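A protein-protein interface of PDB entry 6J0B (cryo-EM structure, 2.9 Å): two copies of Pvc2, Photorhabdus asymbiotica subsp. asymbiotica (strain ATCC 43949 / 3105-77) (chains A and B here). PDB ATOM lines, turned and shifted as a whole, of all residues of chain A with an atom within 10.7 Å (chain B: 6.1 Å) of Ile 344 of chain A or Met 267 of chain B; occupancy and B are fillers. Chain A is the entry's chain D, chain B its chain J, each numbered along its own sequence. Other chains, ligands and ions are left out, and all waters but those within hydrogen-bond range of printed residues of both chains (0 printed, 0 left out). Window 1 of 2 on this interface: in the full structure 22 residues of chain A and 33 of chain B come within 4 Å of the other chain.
The side-chain amide nitrogen of Asn 195 of chain A sits at hydrogen-bond distance from the backbone carbonyl oxygen of Ser 268 of chain B, at 2.9 Å.
The side-chain amide nitrogen (ND2) of Asn 195 of chain A is in hydrogen-bond range of the backbone carbonyl oxygen (O) of Phe 269 of chain B, 3.5 Å away.
ND2 of Asn 195 of chain A lies within hydrogen-bond range of O of Met 271 of chain B, 3.1 Å away.
O of Gly 327 of chain B sits at hydrogen-bond distance from N of Glu 342 of chain A, 3.3 Å away.
The backbone NH of Phe 343 of chain A lies within hydrogen-bond range of the backbone carbonyl oxygen of Gly 327 of chain B (3.3 Å).
The backbone carbonyl oxygen (O) of Phe 343 of chain A lies within hydrogen-bond range of the backbone NH (N) of Met 329 of chain B (3.0 Å).
The backbone carbonyl oxygen of Met 329 of chain B is in hydrogen-bond range of the backbone NH of Ile 345 of chain A.
N of Val 331 of chain B lies within hydrogen-bond range of O of Ile 345 of chain A.
The backbone carbonyl oxygen (O) of Val 331 of chain B lies within hydrogen-bond range of the backbone NH (N) of Gln 347 of chain A (2.8 Å).
O of Glu 342 of chain A lies close to SD of Met 271 of chain B (3.5 Å).
The side-chain hydroxyl of Tyr 249 of chain A lies within hydrogen-bond range of the side-chain carboxylate of Glu 342 of chain A.
OG of Ser 268 of chain B is in hydrogen-bond range of O of Arg 265 of chain B (2.5 Å).
Met 271 of chain B touches Trp 236 of chain A.
Ala 341 of chain A touches Met 271 of chain B (O to C, 3.96 Å).
Met 329 of chain B touches Ala 341 of chain A.
O of Phe 343 of chain A touches CA of Gln 328 of chain B (3.4 Å).
Met 267 of chain B touches Ile 344 of chain A (SD to CG2, 3.6 Å).
OE1 of Gln 328 of chain B touches CD1 of Ile 345 of chain A, at 3.3 Å.
Ile 345 of chain A touches Ile 330 of chain B.
Leu 346 of chain A touches Ile 263 of chain B (CD1 to CG2, 3.7 Å).
O of Val 331 of chain B touches C of Leu 346 of chain A, at 3.7 Å.
CZ of Phe 348 of chain A touches CD1 of Ile 263 of chain B, at 3.5 Å.
Ile 344 of chain A touches just these residues of chain B: Met 267, Ala 270, Met 271 and Met 329.
Of chain A, only Ile 344 and Leu 346 come within 4 Å of Met 267 of chain B.
No residue of chain A comes within 4 Å of Ala 266 of chain B.
Of chain A, only Asn 195 (2.9 Å) comes within 4 Å of Ser 268 of chain B.
Of chain A, only Asn 195 comes within 4 Å of Phe 269 of chain B.
Ala 270 of chain B touches just one residue of chain A: Ile 344.
Of chain A, only Ala 341, Phe 343, Ile 344 and Ile 345 come within 4 Å of Met 329 of chain B.
Printed residues of chain A within 4 Å of Gln 328 of chain B: Phe 343 (3.4 Å) and Ile 345 (3.3 Å).
Of the printed residues of chain A, Gly 327 of chain B touches Ala 341 (3.99 Å), Glu 342 (3.3 Å) and Phe 343 (3.1 Å).
Printed residues of chain B within 4 Å of Asn 195 of chain A: Ser 268, Phe 269 and Met 271.
Of the printed residues of chain B, Ile 345 of chain A touches Gln 328 (3.3 Å), Met 329 (2.6 Å), Ile 330 (3.2 Å) and Val 331 (3.0 Å).
Printed residues of chain B within 4 Å of Trp 236 of chain A: Met 271 (3.5 Å).
The nearest residue of chain A that does not touch Met 267 of chain B is Ile 345 of chain A (5.7 Å).
Printed residues of chain B that touch a printed residue of chain A: Ile 263, Met 267, Ser 268, Phe 269, Ala 270, Met 271, Gly 327, Gln 328, Met 329, Ile 330 and Val 331.
Hydrophobic or aromatic side chains of chain B that line the printed part of chain A: Ile 263, Met 267, Ala 270, Met 271, Met 329 and Ile 330.
Of the 17 printed residues of chain A, 10 touch a printed residue of chain B.
Hydrophobic or aromatic side chains of chain A within 4 Å of the printed part of chain B: Trp 236, Ala 341, Phe 343, Ile 344, Ile 345, Leu 346 and Phe 348.
Among the printed residues, 26 pairs touch across the chains.
Among the printed residues, no Asp or Glu carboxylate lies within 4 Å of a Lys or Arg side-chain nitrogen of the other chain.
No position is printed for both chains.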
ATOM      1  N   ALA A 194     -10.009   4.905  24.605  1.00  0.00           N
ATOM      2  CA  ALA A 194      -9.423   5.746  23.583  1.00  0.00           C
ATOM      3  C   ALA A 194     -10.035   7.145  23.632  1.00  0.00           C
ATOM      4  O   ALA A 194     -10.968   7.406  24.390  1.00  0.00           O
ATOM      5  CB  ALA A 194      -9.595   5.104  22.216  1.00  0.00           C
ATOM      6  N   ASN A 195      -9.470   8.026  22.798  1.00  0.00           N
ATOM      7  CA  ASN A 195      -9.587   9.503  22.780  1.00  0.00           C
ATOM      8  C   ASN A 195      -9.712  10.123  24.182  1.00  0.00           C
ATOM      9  O   ASN A 195     -10.549  10.983  24.467  1.00  0.00           O
ATOM     10  CB  ASN A 195     -10.642   9.995  21.744  1.00  0.00           C
ATOM     11  CG  ASN A 195     -12.111   9.924  22.176  1.00  0.00           C
ATOM     12  OD1 ASN A 195     -12.496   9.289  23.141  1.00  0.00           O
ATOM     13  ND2 ASN A 195     -12.946  10.615  21.413  1.00  0.00           N
ATOM     14  N   ASP A 210      -1.219   8.638   9.664  1.00  0.00           N
ATOM     15  CA  ASP A 210      -2.455   7.860   9.618  1.00  0.00           C
ATOM     16  C   ASP A 210      -2.319   6.625   8.740  1.00  0.00           C
ATOM     17  O   ASP A 210      -2.986   5.616   8.990  1.00  0.00           O
ATOM     18  CB  ASP A 210      -3.604   8.725   9.109  1.00  0.00           C
ATOM     19  CG  ASP A 210      -4.461   9.270  10.225  1.00  0.00           C
ATOM     20  OD1 ASP A 210      -4.451   8.678  11.324  1.00  0.00           O
ATOM     21  OD2 ASP A 210      -5.154  10.283  10.001  1.00  0.00           O
ATOM     22  N   PHE A 228      -2.817  15.265  18.672  1.00  0.00           N
ATOM     23  CA  PHE A 228      -3.783  16.067  17.938  1.00  0.00           C
ATOM     24  C   PHE A 228      -3.647  17.502  18.419  1.00  0.00           C
ATOM     25  O   PHE A 228      -3.391  17.738  19.601  1.00  0.00           O
ATOM     26  CB  PHE A 228      -5.213  15.554  18.155  1.00  0.00           C
ATOM     27  CG  PHE A 228      -5.575  14.366  17.299  1.00  0.00           C
ATOM     28  CD1 PHE A 228      -4.922  13.153  17.445  1.00  0.00           C
ATOM     29  CD2 PHE A 228      -6.587  14.462  16.362  1.00  0.00           C
ATOM     30  CE1 PHE A 228      -5.256  12.069  16.661  1.00  0.00           C
ATOM     31  CE2 PHE A 228      -6.929  13.377  15.577  1.00  0.00           C
ATOM     32  CZ  PHE A 228      -6.259  12.181  15.729  1.00  0.00           C
ATOM     33  N   ASN A 230      -5.787  19.963  18.712  1.00  0.00           N
ATOM     34  CA  ASN A 230      -6.831  20.459  19.599  1.00  0.00           C
ATOM     35  C   ASN A 230      -6.935  19.662  20.891  1.00  0.00           C
ATOM     36  O   ASN A 230      -7.351  20.212  21.916  1.00  0.00           O
ATOM     37  CB  ASN A 230      -8.182  20.455  18.877  1.00  0.00           C
ATOM     38  CG  ASN A 230      -8.571  19.080  18.372  1.00  0.00           C
ATOM     39  OD1 ASN A 230      -7.894  18.505  17.521  1.00  0.00           O
ATOM     40  ND2 ASN A 230      -9.678  18.554  18.882  1.00  0.00           N
ATOM     41  N   THR A 231      -6.555  18.386  20.872  1.00  0.00           N
ATOM     42  CA  THR A 231      -6.675  17.513  22.031  1.00  0.00           C
ATOM     43  C   THR A 231      -5.365  17.350  22.796  1.00  0.00           C
ATOM     44  O   THR A 231      -5.388  16.935  23.960  1.00  0.00           O
ATOM     45  CB  THR A 231      -7.193  16.135  21.586  1.00  0.00           C
ATOM     46  OG1 THR A 231      -8.086  16.303  20.478  1.00  0.00           O
ATOM     47  CG2 THR A 231      -7.950  15.428  22.708  1.00  0.00           C
ATOM     48  N   TRP A 236      -5.449   6.367  20.902  1.00  0.00           N
ATOM     49  CA  TRP A 236      -6.211   6.267  19.666  1.00  0.00           C
ATOM     50  C   TRP A 236      -6.446   4.822  19.251  1.00  0.00           C
ATOM     51  O   TRP A 236      -6.449   4.506  18.060  1.00  0.00           O
ATOM     52  CB  TRP A 236      -5.511   7.039  18.551  1.00  0.00           C
ATOM     53  CG  TRP A 236      -6.422   7.580  17.515  1.00  0.00           C
ATOM     54  CD1 TRP A 236      -6.464   7.231  16.205  1.00  0.00           C
ATOM     55  CD2 TRP A 236      -7.431   8.575  17.701  1.00  0.00           C
ATOM     56  NE1 TRP A 236      -7.435   7.949  15.556  1.00  0.00           N
ATOM     57  CE2 TRP A 236      -8.043   8.781  16.457  1.00  0.00           C
ATOM     58  CE3 TRP A 236      -7.874   9.315  18.800  1.00  0.00           C
ATOM     59  CZ2 TRP A 236      -9.074   9.690  16.280  1.00  0.00           C
ATOM     60  CZ3 TRP A 236      -8.893  10.212  18.622  1.00  0.00           C
ATOM     61  CH2 TRP A 236      -9.480  10.397  17.374  1.00  0.00           C
ATOM     62  N   TYR A 249     -12.126  -5.842  20.778  1.00  0.00           N
ATOM     63  CA  TYR A 249     -11.927  -4.570  21.455  1.00  0.00           C
ATOM     64  C   TYR A 249     -11.617  -4.773  22.932  1.00  0.00           C
ATOM     65  O   TYR A 249     -12.173  -5.670  23.571  1.00  0.00           O
ATOM     66  CB  TYR A 249     -13.164  -3.686  21.306  1.00  0.00           C
ATOM     67  CG  TYR A 249     -13.516  -3.374  19.875  1.00  0.00           C
ATOM     68  CD1 TYR A 249     -12.818  -2.407  19.170  1.00  0.00           C
ATOM     69  CD2 TYR A 249     -14.546  -4.043  19.232  1.00  0.00           C
ATOM     70  CE1 TYR A 249     -13.132  -2.118  17.865  1.00  0.00           C
ATOM     71  CE2 TYR A 249     -14.868  -3.760  17.925  1.00  0.00           C
ATOM     72  CZ  TYR A 249     -14.157  -2.796  17.247  1.00  0.00           C
ATOM     73  OH  TYR A 249     -14.476  -2.508  15.942  1.00  0.00           O
ATOM     74  N   PRO A 340     -17.631  -0.116  20.339  1.00  0.00           N
ATOM     75  CA  PRO A 340     -17.365   1.298  20.063  1.00  0.00           C
ATOM     76  C   PRO A 340     -17.354   1.608  18.574  1.00  0.00           C
ATOM     77  O   PRO A 340     -16.925   0.808  17.743  1.00  0.00           O
ATOM     78  CB  PRO A 340     -15.976   1.508  20.679  1.00  0.00           C
ATOM     79  CG  PRO A 340     -15.326   0.195  20.567  1.00  0.00           C
ATOM     80  CD  PRO A 340     -16.407  -0.836  20.732  1.00  0.00           C
ATOM     81  N   ALA A 341     -17.852   2.796  18.240  1.00  0.00           N
ATOM     82  CA  ALA A 341     -17.770   3.293  16.873  1.00  0.00           C
ATOM     83  C   ALA A 341     -16.342   3.706  16.574  1.00  0.00           C
ATOM     84  O   ALA A 341     -15.811   4.625  17.205  1.00  0.00           O
ATOM     85  CB  ALA A 341     -18.713   4.473  16.677  1.00  0.00           C
ATOM     86  N   GLU A 342     -15.715   3.043  15.613  1.00  0.00           N
ATOM     87  CA  GLU A 342     -14.296   3.242  15.367  1.00  0.00           C
ATOM     88  C   GLU A 342     -14.000   4.084  14.140  1.00  0.00           C
ATOM     89  O   GLU A 342     -13.042   4.854  14.151  1.00  0.00           O
ATOM     90  CB  GLU A 342     -13.600   1.890  15.232  1.00  0.00           C
ATOM     91  CG  GLU A 342     -12.166   1.914  15.679  1.00  0.00           C
ATOM     92  CD  GLU A 342     -11.546   0.546  15.659  1.00  0.00           C
ATOM     93  OE1 GLU A 342     -10.350   0.425  15.999  1.00  0.00           O
ATOM     94  OE2 GLU A 342     -12.249  -0.417  15.291  1.00  0.00           O
ATOM     95  N   PHE A 343     -14.793   3.962  13.082  1.00  0.00           N
ATOM     96  CA  PHE A 343     -14.621   4.754  11.875  1.00  0.00           C
ATOM     97  C   PHE A 343     -15.852   5.620  11.662  1.00  0.00           C
ATOM     98  O   PHE A 343     -16.979   5.163  11.861  1.00  0.00           O
ATOM     99  CB  PHE A 343     -14.404   3.865  10.652  1.00  0.00           C
ATOM    100  CG  PHE A 343     -13.656   2.601  10.946  1.00  0.00           C
ATOM    101  CD1 PHE A 343     -12.294   2.624  11.165  1.00  0.00           C
ATOM    102  CD2 PHE A 343     -14.313   1.386  10.994  1.00  0.00           C
ATOM    103  CE1 PHE A 343     -11.598   1.465  11.434  1.00  0.00           C
ATOM    104  CE2 PHE A 343     -13.625   0.223  11.261  1.00  0.00           C
ATOM    105  CZ  PHE A 343     -12.264   0.265  11.482  1.00  0.00           C
ATOM    106  N   ILE A 344     -15.639   6.870  11.267  1.00  0.00           N
ATOM    107  CA  ILE A 344     -16.724   7.768  10.896  1.00  0.00           C
ATOM    108  C   ILE A 344     -16.447   8.276   9.491  1.00  0.00           C
ATOM    109  O   ILE A 344     -15.393   8.862   9.235  1.00  0.00           O
ATOM    110  CB  ILE A 344     -16.884   8.931  11.884  1.00  0.00           C
ATOM    111  CG1 ILE A 344     -17.499   8.435  13.191  1.00  0.00           C
ATOM    112  CG2 ILE A 344     -17.791   9.975  11.302  1.00  0.00           C
ATOM    113  CD1 ILE A 344     -17.843   9.546  14.182  1.00  0.00           C
ATOM    114  N   ILE A 345     -17.388   8.052   8.581  1.00  0.00           N
ATOM    115  CA  ILE A 345     -17.211   8.378   7.175  1.00  0.00           C
ATOM    116  C   ILE A 345     -18.097   9.565   6.838  1.00  0.00           C
ATOM    117  O   ILE A 345     -19.324   9.481   6.932  1.00  0.00           O
ATOM    118  CB  ILE A 345     -17.531   7.174   6.282  1.00  0.00           C
ATOM    119  CG1 ILE A 345     -16.590   6.024   6.624  1.00  0.00           C
ATOM    120  CG2 ILE A 345     -17.411   7.553   4.826  1.00  0.00           C
ATOM    121  CD1 ILE A 345     -16.972   4.731   5.993  1.00  0.00           C
ATOM    122  N   LEU A 346     -17.477  10.669   6.445  1.00  0.00           N
ATOM    123  CA  LEU A 346     -18.174  11.872   6.016  1.00  0.00           C
ATOM    124  C   LEU A 346     -18.277  11.865   4.507  1.00  0.00           C
ATOM    125  O   LEU A 346     -17.276  11.647   3.824  1.00  0.00           O
ATOM    126  CB  LEU A 346     -17.420  13.120   6.440  1.00  0.00           C
ATOM    127  CG  LEU A 346     -17.545  13.573   7.860  1.00  0.00           C
ATOM    128  CD1 LEU A 346     -16.348  14.440   8.167  1.00  0.00           C
ATOM    129  CD2 LEU A 346     -18.815  14.359   7.923  1.00  0.00           C
ATOM    130  N   GLN A 347     -19.467  12.130   3.990  1.00  0.00           N
ATOM    131  CA  GLN A 347     -19.652  12.367   2.570  1.00  0.00           C
ATOM    132  C   GLN A 347     -20.077  13.811   2.370  1.00  0.00           C
ATOM    133  O   GLN A 347     -21.125  14.228   2.870  1.00  0.00           O
ATOM    134  CB  GLN A 347     -20.670  11.406   1.976  1.00  0.00           C
ATOM    135  CG  GLN A 347     -20.099  10.036   1.762  1.00  0.00           C
ATOM    136  CD  GLN A 347     -20.993   8.973   2.308  1.00  0.00           C
ATOM    137  OE1 GLN A 347     -22.115   9.254   2.711  1.00  0.00           O
ATOM    138  NE2 GLN A 347     -20.509   7.740   2.330  1.00  0.00           N
ATOM    139  N   PHE A 348     -19.257  14.571   1.657  1.00  0.00           N
ATOM    140  CA  PHE A 348     -19.519  15.977   1.398  1.00  0.00           C
ATOM    141  C   PHE A 348     -20.018  16.132  -0.028  1.00  0.00           C
ATOM    142  O   PHE A 348     -19.321  15.765  -0.978  1.00  0.00           O
ATOM    143  CB  PHE A 348     -18.274  16.823   1.646  1.00  0.00           C
ATOM    144  CG  PHE A 348     -18.072  17.165   3.082  1.00  0.00           C
ATOM    145  CD1 PHE A 348     -17.497  16.255   3.943  1.00  0.00           C
ATOM    146  CD2 PHE A 348     -18.481  18.387   3.581  1.00  0.00           C
ATOM    147  CE1 PHE A 348     -17.321  16.559   5.271  1.00  0.00           C
ATOM    148  CE2 PHE A 348     -18.302  18.694   4.909  1.00  0.00           C
ATOM    149  CZ  PHE A 348     -17.717  17.775   5.750  1.00  0.00           C
ATOM    150  N   ASP B 262     -12.884  21.456  10.144  1.00  0.00           N
ATOM    151  CA  ASP B 262     -13.587  21.796  11.376  1.00  0.00           C
ATOM    152  C   ASP B 262     -14.583  20.712  11.761  1.00  0.00           C
ATOM    153  O   ASP B 262     -14.834  20.483  12.949  1.00  0.00           O
ATOM    154  CB  ASP B 262     -14.299  23.131  11.226  1.00  0.00           C
ATOM    155  CG  ASP B 262     -13.355  24.262  10.899  1.00  0.00           C
ATOM    156  OD1 ASP B 262     -12.137  24.017  10.817  1.00  0.00           O
ATOM    157  OD2 ASP B 262     -13.832  25.403  10.725  1.00  0.00           O
ATOM    158  N   ILE B 263     -15.163  20.037  10.769  1.00  0.00           N
ATOM    159  CA  ILE B 263     -16.066  18.925  11.047  1.00  0.00           C
ATOM    160  C   ILE B 263     -15.274  17.712  11.528  1.00  0.00           C
ATOM    161  O   ILE B 263     -15.761  16.919  12.344  1.00  0.00           O
ATOM    162  CB  ILE B 263     -16.926  18.643   9.796  1.00  0.00           C
ATOM    163  CG1 ILE B 263     -17.898  19.805   9.590  1.00  0.00           C
ATOM    164  CG2 ILE B 263     -17.718  17.354   9.893  1.00  0.00           C
ATOM    165  CD1 ILE B 263     -18.833  19.654   8.424  1.00  0.00           C
ATOM    166  N   LYS B 264     -14.016  17.591  11.078  1.00  0.00           N
ATOM    167  CA  LYS B 264     -13.092  16.582  11.602  1.00  0.00           C
ATOM    168  C   LYS B 264     -12.906  16.710  13.105  1.00  0.00           C
ATOM    169  O   LYS B 264     -12.829  15.703  13.816  1.00  0.00           O
ATOM    170  CB  LYS B 264     -11.724  16.720  10.938  1.00  0.00           C
ATOM    171  CG  LYS B 264     -11.367  15.731   9.893  1.00  0.00           C
ATOM    172  CD  LYS B 264      -9.932  15.260  10.079  1.00  0.00           C
ATOM    173  CE  LYS B 264      -9.494  14.305   8.981  1.00  0.00           C
ATOM    174  NZ  LYS B 264      -8.114  13.796   9.168  1.00  0.00           N
ATOM    175  N   ARG B 265     -12.830  17.942  13.608  1.00  0.00           N
ATOM    176  CA  ARG B 265     -12.596  18.141  15.031  1.00  0.00           C
ATOM    177  C   ARG B 265     -13.848  17.848  15.846  1.00  0.00           C
ATOM    178  O   ARG B 265     -13.757  17.361  16.978  1.00  0.00           O
ATOM    179  CB  ARG B 265     -12.106  19.562  15.284  1.00  0.00           C
ATOM    180  CG  ARG B 265     -10.799  19.873  14.592  1.00  0.00           C
ATOM    181  CD  ARG B 265     -10.307  21.254  14.952  1.00  0.00           C
ATOM    182  NE  ARG B 265      -9.069  21.583  14.255  1.00  0.00           N
ATOM    183  CZ  ARG B 265      -8.423  22.735  14.392  1.00  0.00           C
ATOM    184  NH1 ARG B 265      -8.898  23.671  15.202  1.00  0.00           N
ATOM    185  NH2 ARG B 265      -7.303  22.952  13.719  1.00  0.00           N
ATOM    186  N   ALA B 266     -15.026  18.129  15.291  1.00  0.00           N
ATOM    187  CA  ALA B 266     -16.261  17.794  15.992  1.00  0.00           C
ATOM    188  C   ALA B 266     -16.532  16.295  15.946  1.00  0.00           C
ATOM    189  O   ALA B 266     -17.197  15.744  16.822  1.00  0.00           O
ATOM    190  CB  ALA B 266     -17.433  18.571  15.401  1.00  0.00           C
ATOM    191  N   MET B 267     -16.028  15.603  14.939  1.00  0.00           N
ATOM    192  CA  MET B 267     -16.221  14.165  14.970  1.00  0.00           C
ATOM    193  C   MET B 267     -15.124  13.462  15.737  1.00  0.00           C
ATOM    194  O   MET B 267     -15.152  12.234  15.854  1.00  0.00           O
ATOM    195  CB  MET B 267     -16.320  13.641  13.565  1.00  0.00           C
ATOM    196  CG  MET B 267     -17.504  14.203  12.916  1.00  0.00           C
ATOM    197  SD  MET B 267     -17.541  13.524  11.308  1.00  0.00           S
ATOM    198  CE  MET B 267     -19.276  13.302  11.199  1.00  0.00           C
ATOM    199  N   SER B 268     -14.165  14.217  16.267  1.00  0.00           N
ATOM    200  CA  SER B 268     -13.131  13.611  17.087  1.00  0.00           C
ATOM    201  C   SER B 268     -13.689  13.158  18.428  1.00  0.00           C
ATOM    202  O   SER B 268     -13.227  12.156  18.984  1.00  0.00           O
ATOM    203  CB  SER B 268     -11.981  14.591  17.293  1.00  0.00           C
ATOM    204  OG  SER B 268     -12.368  15.631  18.170  1.00  0.00           O
ATOM    205  N   PHE B 269     -14.689  13.866  18.967  1.00  0.00           N
ATOM    206  CA  PHE B 269     -15.206  13.456  20.271  1.00  0.00           C
ATOM    207  C   PHE B 269     -16.106  12.234  20.149  1.00  0.00           C
ATOM    208  O   PHE B 269     -16.291  11.494  21.119  1.00  0.00           O
ATOM    209  CB  PHE B 269     -15.911  14.615  21.011  1.00  0.00           C
ATOM    210  CG  PHE B 269     -17.117  15.240  20.313  1.00  0.00           C
ATOM    211  CD1 PHE B 269     -18.349  14.587  20.228  1.00  0.00           C
ATOM    212  CD2 PHE B 269     -17.047  16.554  19.874  1.00  0.00           C
ATOM    213  CE1 PHE B 269     -19.436  15.183  19.630  1.00  0.00           C
ATOM    214  CE2 PHE B 269     -18.153  17.173  19.303  1.00  0.00           C
ATOM    215  CZ  PHE B 269     -19.337  16.470  19.165  1.00  0.00           C
ATOM    216  N   ALA B 270     -16.669  12.004  18.963  1.00  0.00           N
ATOM    217  CA  ALA B 270     -17.520  10.842  18.760  1.00  0.00           C
ATOM    218  C   ALA B 270     -16.722   9.565  18.565  1.00  0.00           C
ATOM    219  O   ALA B 270     -17.321   8.490  18.490  1.00  0.00           O
ATOM    220  CB  ALA B 270     -18.425  11.055  17.553  1.00  0.00           C
ATOM    221  N   MET B 271     -15.398   9.669  18.454  1.00  0.00           N
ATOM    222  CA  MET B 271     -14.545   8.502  18.304  1.00  0.00           C
ATOM    223  C   MET B 271     -14.632   7.605  19.525  1.00  0.00           C
ATOM    224  O   MET B 271     -14.581   8.076  20.664  1.00  0.00           O
ATOM    225  CB  MET B 271     -13.096   8.932  18.095  1.00  0.00           C
ATOM    226  CG  MET B 271     -12.758   9.294  16.690  1.00  0.00           C
ATOM    227  SD  MET B 271     -13.302   8.031  15.564  1.00  0.00           S
ATOM    228  CE  MET B 271     -14.374   9.079  14.642  1.00  0.00           C
ATOM    229  N   VAL B 283     -23.759  13.675  16.962  1.00  0.00           N
ATOM    230  CA  VAL B 283     -22.908  13.970  15.817  1.00  0.00           C
ATOM    231  C   VAL B 283     -23.608  14.938  14.874  1.00  0.00           C
ATOM    232  O   VAL B 283     -22.995  15.885  14.367  1.00  0.00           O
ATOM    233  CB  VAL B 283     -22.523  12.660  15.108  1.00  0.00           C
ATOM    234  CG1 VAL B 283     -21.759  12.932  13.855  1.00  0.00           C
ATOM    235  CG2 VAL B 283     -21.691  11.804  16.014  1.00  0.00           C
ATOM    236  N   ILE B 287     -22.567  19.083  14.054  1.00  0.00           N
ATOM    237  CA  ILE B 287     -22.321  19.605  12.715  1.00  0.00           C
ATOM    238  C   ILE B 287     -23.320  20.701  12.379  1.00  0.00           C
ATOM    239  O   ILE B 287     -22.968  21.711  11.759  1.00  0.00           O
ATOM    240  CB  ILE B 287     -22.364  18.459  11.692  1.00  0.00           C
ATOM    241  CG1 ILE B 287     -21.272  17.446  11.999  1.00  0.00           C
ATOM    242  CG2 ILE B 287     -22.200  18.971  10.274  1.00  0.00           C
ATOM    243  CD1 ILE B 287     -21.236  16.339  11.021  1.00  0.00           C
ATOM    244  N   ILE B 313     -27.910  11.743   9.055  1.00  0.00           N
ATOM    245  CA  ILE B 313     -27.458  10.512   9.691  1.00  0.00           C
ATOM    246  C   ILE B 313     -28.684   9.649   9.952  1.00  0.00           C
ATOM    247  O   ILE B 313     -29.774  10.162  10.216  1.00  0.00           O
ATOM    248  CB  ILE B 313     -26.698  10.764  11.014  1.00  0.00           C
ATOM    249  CG1 ILE B 313     -25.859  12.033  10.938  1.00  0.00           C
ATOM    250  CG2 ILE B 313     -25.799   9.593  11.352  1.00  0.00           C
ATOM    251  CD1 ILE B 313     -24.989  12.249  12.141  1.00  0.00           C
ATOM    252  N   GLY B 327     -18.571  -1.141  12.473  1.00  0.00           N
ATOM    253  CA  GLY B 327     -18.051  -0.011  13.214  1.00  0.00           C
ATOM    254  C   GLY B 327     -18.119   1.308  12.484  1.00  0.00           C
ATOM    255  O   GLY B 327     -17.615   2.307  13.008  1.00  0.00           O
ATOM    256  N   GLN B 328     -18.725   1.352  11.304  1.00  0.00           N
ATOM    257  CA  GLN B 328     -18.747   2.568  10.510  1.00  0.00           C
ATOM    258  C   GLN B 328     -19.920   3.456  10.902  1.00  0.00           C
ATOM    259  O   GLN B 328     -20.949   2.987  11.389  1.00  0.00           O
ATOM    260  CB  GLN B 328     -18.829   2.233   9.022  1.00  0.00           C
ATOM    261  CG  GLN B 328     -17.731   1.319   8.537  1.00  0.00           C
ATOM    262  CD  GLN B 328     -17.896   0.942   7.084  1.00  0.00           C
ATOM    263  OE1 GLN B 328     -18.379   1.731   6.278  1.00  0.00           O
ATOM    264  NE2 GLN B 328     -17.501  -0.276   6.743  1.00  0.00           N
ATOM    265  N   MET B 329     -19.745   4.756  10.684  1.00  0.00           N
ATOM    266  CA  MET B 329     -20.788   5.748  10.907  1.00  0.00           C
ATOM    267  C   MET B 329     -20.729   6.735   9.757  1.00  0.00           C
ATOM    268  O   MET B 329     -19.707   7.397   9.564  1.00  0.00           O
ATOM    269  CB  MET B 329     -20.597   6.462  12.245  1.00  0.00           C
ATOM    270  CG  MET B 329     -21.627   7.530  12.523  1.00  0.00           C
ATOM    271  SD  MET B 329     -21.297   8.442  14.038  1.00  0.00           S
ATOM    272  CE  MET B 329     -20.877   7.110  15.150  1.00  0.00           C
ATOM    273  N   ILE B 330     -21.807   6.833   8.988  1.00  0.00           N
ATOM    274  CA  ILE B 330     -21.813   7.578   7.738  1.00  0.00           C
ATOM    275  C   ILE B 330     -22.719   8.793   7.871  1.00  0.00           C
ATOM    276  O   ILE B 330     -23.883   8.668   8.268  1.00  0.00           O
ATOM    277  CB  ILE B 330     -22.250   6.692   6.565  1.00  0.00           C
ATOM    278  CG1 ILE B 330     -21.329   5.478   6.468  1.00  0.00           C
ATOM    279  CG2 ILE B 330     -22.222   7.483   5.296  1.00  0.00           C
ATOM    280  CD1 ILE B 330     -21.472   4.698   5.194  1.00  0.00           C
ATOM    281  N   VAL B 331     -22.173   9.969   7.558  1.00  0.00           N
ATOM    282  CA  VAL B 331     -22.883  11.241   7.572  1.00  0.00           C
ATOM    283  C   VAL B 331     -22.799  11.840   6.176  1.00  0.00           C
ATOM    284  O   VAL B 331     -21.790  11.687   5.482  1.00  0.00           O
ATOM    285  CB  VAL B 331     -22.281  12.196   8.629  1.00  0.00           C
ATOM    286  CG1 VAL B 331     -23.125  13.442   8.825  1.00  0.00           C
ATOM    287  CG2 VAL B 331     -22.130  11.481   9.939  1.00  0.00           C
